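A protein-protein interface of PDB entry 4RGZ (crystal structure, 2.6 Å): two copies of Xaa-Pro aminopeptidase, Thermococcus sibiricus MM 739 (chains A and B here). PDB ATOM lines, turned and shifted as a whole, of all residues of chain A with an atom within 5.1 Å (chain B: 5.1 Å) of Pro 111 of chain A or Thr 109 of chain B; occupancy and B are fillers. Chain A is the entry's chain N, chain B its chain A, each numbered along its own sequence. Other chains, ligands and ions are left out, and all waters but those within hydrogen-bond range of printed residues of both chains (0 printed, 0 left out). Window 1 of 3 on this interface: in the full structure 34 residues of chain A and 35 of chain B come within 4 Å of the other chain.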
ATOM      1  N   THR A 109      -7.911 -11.179 -21.645  1.00  0.00           N
ATOM      2  CA  THR A 109      -9.284 -11.543 -21.231  1.00  0.00           C
ATOM      3  C   THR A 109     -10.378 -11.205 -22.245  1.00  0.00           C
ATOM      4  O   THR A 109     -11.257 -12.021 -22.511  1.00  0.00           O
ATOM      5  CB  THR A 109      -9.688 -10.871 -19.893  1.00  0.00           C
ATOM      6  OG1 THR A 109     -10.102  -9.519 -20.139  1.00  0.00           O
ATOM      7  CG2 THR A 109      -8.541 -10.889 -18.872  1.00  0.00           C
ATOM      8  N   MET A 110     -10.310  -9.997 -22.796  1.00  0.00           N
ATOM      9  CA  MET A 110     -11.369  -9.443 -23.628  1.00  0.00           C
ATOM     10  C   MET A 110     -11.442 -10.051 -25.039  1.00  0.00           C
ATOM     11  O   MET A 110     -10.411 -10.200 -25.704  1.00  0.00           O
ATOM     12  CB  MET A 110     -11.226  -7.908 -23.671  1.00  0.00           C
ATOM     13  CG  MET A 110     -11.416  -7.233 -25.022  1.00  0.00           C
ATOM     14  SD  MET A 110     -10.379  -5.764 -25.147  1.00  0.00           S
ATOM     15  CE  MET A 110     -10.548  -5.350 -26.881  1.00  0.00           C
ATOM     16  N   PRO A 111     -12.666 -10.426 -25.481  1.00  0.00           N
ATOM     17  CA  PRO A 111     -12.990 -10.750 -26.885  1.00  0.00           C
ATOM     18  C   PRO A 111     -12.522  -9.695 -27.902  1.00  0.00           C
ATOM     19  O   PRO A 111     -12.551  -8.502 -27.591  1.00  0.00           O
ATOM     20  CB  PRO A 111     -14.521 -10.828 -26.868  1.00  0.00           C
ATOM     21  CG  PRO A 111     -14.838 -11.341 -25.496  1.00  0.00           C
ATOM     22  CD  PRO A 111     -13.752 -10.846 -24.567  1.00  0.00           C
ATOM     23  N   VAL A 112     -12.104 -10.144 -29.094  1.00  0.00           N
ATOM     24  CA  VAL A 112     -11.614  -9.256 -30.165  1.00  0.00           C
ATOM     25  C   VAL A 112     -12.721  -8.312 -30.557  1.00  0.00           C
ATOM     26  O   VAL A 112     -12.893  -7.286 -29.917  1.00  0.00           O
ATOM     27  CB  VAL A 112     -11.131 -10.001 -31.433  1.00  0.00           C
ATOM     28  CG1 VAL A 112     -10.413  -9.037 -32.361  1.00  0.00           C
ATOM     29  CG2 VAL A 112     -10.195 -11.141 -31.085  1.00  0.00           C
ATOM     30  N   GLY A 113     -13.458  -8.679 -31.603  1.00  0.00           N
ATOM     31  CA  GLY A 113     -14.654  -7.971 -32.079  1.00  0.00           C
ATOM     32  C   GLY A 113     -14.787  -6.505 -31.730  1.00  0.00           C
ATOM     33  O   GLY A 113     -14.727  -5.644 -32.607  1.00  0.00           O
ATOM     34  N   VAL A 114     -14.996  -6.233 -30.441  1.00  0.00           N
ATOM     35  CA  VAL A 114     -14.915  -4.883 -29.886  1.00  0.00           C
ATOM     36  C   VAL A 114     -13.608  -4.281 -30.382  1.00  0.00           C
ATOM     37  O   VAL A 114     -13.164  -3.244 -29.904  1.00  0.00           O
ATOM     38  CB  VAL A 114     -14.885  -4.863 -28.330  1.00  0.00           C
ATOM     39  CG1 VAL A 114     -15.804  -3.768 -27.798  1.00  0.00           C
ATOM     40  CG2 VAL A 114     -15.235  -6.222 -27.707  1.00  0.00           C
ATOM     41  N   ALA B  27     -14.311 -19.723 -31.887  1.00  0.00           N
ATOM     42  CA  ALA B  27     -13.646 -19.917 -30.594  1.00  0.00           C
ATOM     43  C   ALA B  27     -14.649 -20.394 -29.520  1.00  0.00           C
ATOM     44  O   ALA B  27     -15.840 -20.495 -29.812  1.00  0.00           O
ATOM     45  CB  ALA B  27     -12.954 -18.624 -30.174  1.00  0.00           C
ATOM     46  N   PRO B  28     -14.173 -20.727 -28.291  1.00  0.00           N
ATOM     47  CA  PRO B  28     -15.078 -20.932 -27.152  1.00  0.00           C
ATOM     48  C   PRO B  28     -16.013 -19.758 -26.908  1.00  0.00           C
ATOM     49  O   PRO B  28     -15.617 -18.608 -27.080  1.00  0.00           O
ATOM     50  CB  PRO B  28     -14.111 -21.095 -25.976  1.00  0.00           C
ATOM     51  CG  PRO B  28     -12.950 -21.810 -26.599  1.00  0.00           C
ATOM     52  CD  PRO B  28     -12.819 -21.246 -27.989  1.00  0.00           C
ATOM     53  N   GLY B  29     -17.241 -20.061 -26.507  1.00  0.00           N
ATOM     54  CA  GLY B  29     -18.275 -19.044 -26.352  1.00  0.00           C
ATOM     55  C   GLY B  29     -19.586 -19.370 -27.066  1.00  0.00           C
ATOM     56  O   GLY B  29     -19.754 -20.481 -27.580  1.00  0.00           O
ATOM     57  N   SER B  30     -20.496 -18.390 -27.133  1.00  0.00           N
ATOM     58  CA  SER B  30     -21.867 -18.610 -27.612  1.00  0.00           C
ATOM     59  C   SER B  30     -21.980 -19.236 -29.000  1.00  0.00           C
ATOM     60  O   SER B  30     -22.839 -20.075 -29.246  1.00  0.00           O
ATOM     61  CB  SER B  30     -22.667 -17.304 -27.581  1.00  0.00           C
ATOM     62  OG  SER B  30     -22.549 -16.663 -26.330  1.00  0.00           O
ATOM     63  N   ASN B  31     -21.117 -18.809 -29.905  1.00  0.00           N
ATOM     64  CA  ASN B  31     -21.102 -19.347 -31.243  1.00  0.00           C
ATOM     65  C   ASN B  31     -20.655 -20.792 -31.360  1.00  0.00           C
ATOM     66  O   ASN B  31     -21.229 -21.532 -32.157  1.00  0.00           O
ATOM     67  CB  ASN B  31     -20.260 -18.459 -32.128  1.00  0.00           C
ATOM     68  CG  ASN B  31     -20.871 -17.099 -32.283  1.00  0.00           C
ATOM     69  OD1 ASN B  31     -22.096 -16.977 -32.336  1.00  0.00           O
ATOM     70  ND2 ASN B  31     -20.033 -16.064 -32.332  1.00  0.00           N
ATOM     71  N   ASP B 107     -14.431 -15.326 -35.248  1.00  0.00           N
ATOM     72  CA  ASP B 107     -15.398 -15.327 -34.141  1.00  0.00           C
ATOM     73  C   ASP B 107     -15.105 -14.212 -33.138  1.00  0.00           C
ATOM     74  O   ASP B 107     -14.149 -14.293 -32.381  1.00  0.00           O
ATOM     75  CB  ASP B 107     -15.402 -16.703 -33.452  1.00  0.00           C
ATOM     76  CG  ASP B 107     -16.258 -16.743 -32.193  1.00  0.00           C
ATOM     77  OD1 ASP B 107     -15.732 -16.419 -31.121  1.00  0.00           O
ATOM     78  OD2 ASP B 107     -17.441 -17.127 -32.261  1.00  0.00           O
ATOM     79  N   ASP B 108     -15.930 -13.170 -33.161  1.00  0.00           N
ATOM     80  CA  ASP B 108     -15.905 -12.073 -32.177  1.00  0.00           C
ATOM     81  C   ASP B 108     -15.417 -12.484 -30.780  1.00  0.00           C
ATOM     82  O   ASP B 108     -14.436 -11.934 -30.274  1.00  0.00           O
ATOM     83  CB  ASP B 108     -17.301 -11.424 -32.062  1.00  0.00           C
ATOM     84  CG  ASP B 108     -17.720 -10.657 -33.333  1.00  0.00           C
ATOM     85  OD1 ASP B 108     -17.769 -11.241 -34.440  1.00  0.00           O
ATOM     86  OD2 ASP B 108     -18.052  -9.456 -33.214  1.00  0.00           O
ATOM     87  N   THR B 109     -16.092 -13.466 -30.185  1.00  0.00           N
ATOM     88  CA  THR B 109     -15.793 -13.934 -28.820  1.00  0.00           C
ATOM     89  C   THR B 109     -14.362 -14.452 -28.570  1.00  0.00           C
ATOM     90  O   THR B 109     -13.994 -14.692 -27.415  1.00  0.00           O
ATOM     91  CB  THR B 109     -16.818 -15.001 -28.324  1.00  0.00           C
ATOM     92  OG1 THR B 109     -16.568 -16.276 -28.941  1.00  0.00           O
ATOM     93  CG2 THR B 109     -18.286 -14.560 -28.575  1.00  0.00           C
ATOM     94  N   MET B 110     -13.566 -14.628 -29.634  1.00  0.00           N
ATOM     95  CA  MET B 110     -12.143 -14.982 -29.500  1.00  0.00           C
ATOM     96  C   MET B 110     -11.453 -13.846 -28.762  1.00  0.00           C
ATOM     97  O   MET B 110     -11.769 -12.685 -29.019  1.00  0.00           O
ATOM     98  CB  MET B 110     -11.477 -15.202 -30.867  1.00  0.00           C
ATOM     99  CG  MET B 110      -9.962 -14.984 -30.881  1.00  0.00           C
ATOM    100  SD  MET B 110      -9.092 -15.478 -32.389  1.00  0.00           S
ATOM    101  CE  MET B 110      -9.409 -17.239 -32.399  1.00  0.00           C
ATOM    102  N   PRO B 111     -10.522 -14.170 -27.837  1.00  0.00           N
ATOM    103  CA  PRO B 111      -9.893 -13.109 -27.056  1.00  0.00           C
ATOM    104  C   PRO B 111      -8.653 -12.507 -27.737  1.00  0.00           C
ATOM    105  O   PRO B 111      -7.911 -13.226 -28.418  1.00  0.00           O
ATOM    106  CB  PRO B 111      -9.520 -13.822 -25.758  1.00  0.00           C
ATOM    107  CG  PRO B 111      -9.321 -15.254 -26.141  1.00  0.00           C
ATOM    108  CD  PRO B 111     -10.031 -15.506 -27.443  1.00  0.00           C
ATOM    109  N   VAL B 112      -8.444 -11.200 -27.564  1.00  0.00           N
ATOM    110  CA  VAL B 112      -7.257 -10.527 -28.119  1.00  0.00           C
ATOM    111  C   VAL B 112      -6.027 -10.847 -27.276  1.00  0.00           C
ATOM    112  O   VAL B 112      -5.668 -10.120 -26.352  1.00  0.00           O
ATOM    113  CB  VAL B 112      -7.401  -8.990 -28.235  1.00  0.00           C
ATOM    114  CG1 VAL B 112      -6.529  -8.470 -29.379  1.00  0.00           C
ATOM    115  CG2 VAL B 112      -8.854  -8.569 -28.422  1.00  0.00           C
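Printed residues of chain A that touch a printed residue of chain B: Met 110, Pro 111, Val 112 and Gly 113. Hydrophobic or aromatic side chains of chain A within 4 Å of the printed part of chain B: Met 110, Pro 111 and Val 112. Hydrophobic or aromatic side chains of chain B that line the printed part of chain A: Met 110, Pro 111 and Val 112.
Met 110 of chain A touches Pro 111 of chain B, and with the chains exchanged Pro 111 of chain A touches Met 110 of chain B. Pro 111 of chain A touches Thr 109 of chain B, but with the chains exchanged Thr 109 of chain A does not touch Pro 111 of chain B (4.1 Å). Pro 111 of chain B touches its own counterpart, Pro 111 of chain A. Pro 111 of chain A touches Val 112 of chain B, and with the chains exchanged Val 112 of chain A touches Pro 111 of chain B. 4 positions are printed for both chains. Of the 12 pairs that touch across the chains among the printed residues, 8 have their exchanged pair printed and touching as well.
Among the printed residues, merely in contact across the chains: Pro 111 of chain A with Met 110 of chain B, Met 110 of chain A with Pro 111 of chain B, Val 112 of chain A with Val 112 of chain B, Pro 111 of chain A with Asp 108 of chain B, Gly 113 of chain A with Asp 108 of chain B, Pro 111 of chain A with Val 112 of chain B, Pro 111 of chain A with Thr 109 of chain B, Pro 111 of chain A with Pro 111 of chain B and Val 112 of chain A with Pro 111 of chain B.
Pro 111 of chain A touches just these residues of chain B: Asp 108, Thr 109, Met 110, Pro 111 and Val 112. Of chain A, only Pro 111 (3.9 Å) comes within 4 Å of Thr 109 of chain B. Printed residues of chain A within 4 Å of Asp 108 of chain B: Pro 111, Val 112 and Gly 113. Of the printed residues of chain A, Met 110 of chain B touches Pro 111 and Val 112. Printed residues of chain B within 4 Å of Gly 113 of chain A: Asp 108 (3.6 Å). Of the printed residues of chain B, Met 110 of chain A touches Pro 111 (3.2 Å) and Val 112 (2.9 Å). Of the printed residues of chain A, Val 112 of chain B touches Met 110, Pro 111 and Val 112. Pro 28 of chain B touches none of the printed residues of chain A. Thr 109 of chain A touches none of the printed residues of chain B. The nearest printed residue of chain B that does not touch Pro 111 of chain A is Asp 107 of chain B (6.5 Å). The nearest residue of chain A that does not touch Thr 109 of chain B is Val 112 of chain A (4.9 Å).
The backbone carbonyl oxygen (O) of Pro 28 of chain B lies within hydrogen-bond range of the side-chain hydroxyl (OG1) of Thr 109 of chain B, 3.1 Å away. OD1 of Asp 107 of chain B is in hydrogen-bond range of N of Thr 109 of chain B. The side-chain carboxylate (OD1) of Asp 107 of chain B is in hydrogen-bond range of the backbone NH (N) of Met 110 of chain B (3.2 Å).
The backbone NH (N) of Val 112 of chain A sits at hydrogen-bond distance from the backbone carbonyl oxygen (O) of Asp 108 of chain B (3.2 Å). The backbone carbonyl oxygen (O) of Met 110 of chain B lies within hydrogen-bond range of the backbone NH (N) of Val 112 of chain A. O of Met 110 of chain A lies within hydrogen-bond range of N of Val 112 of chain B, 2.9 Å away.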
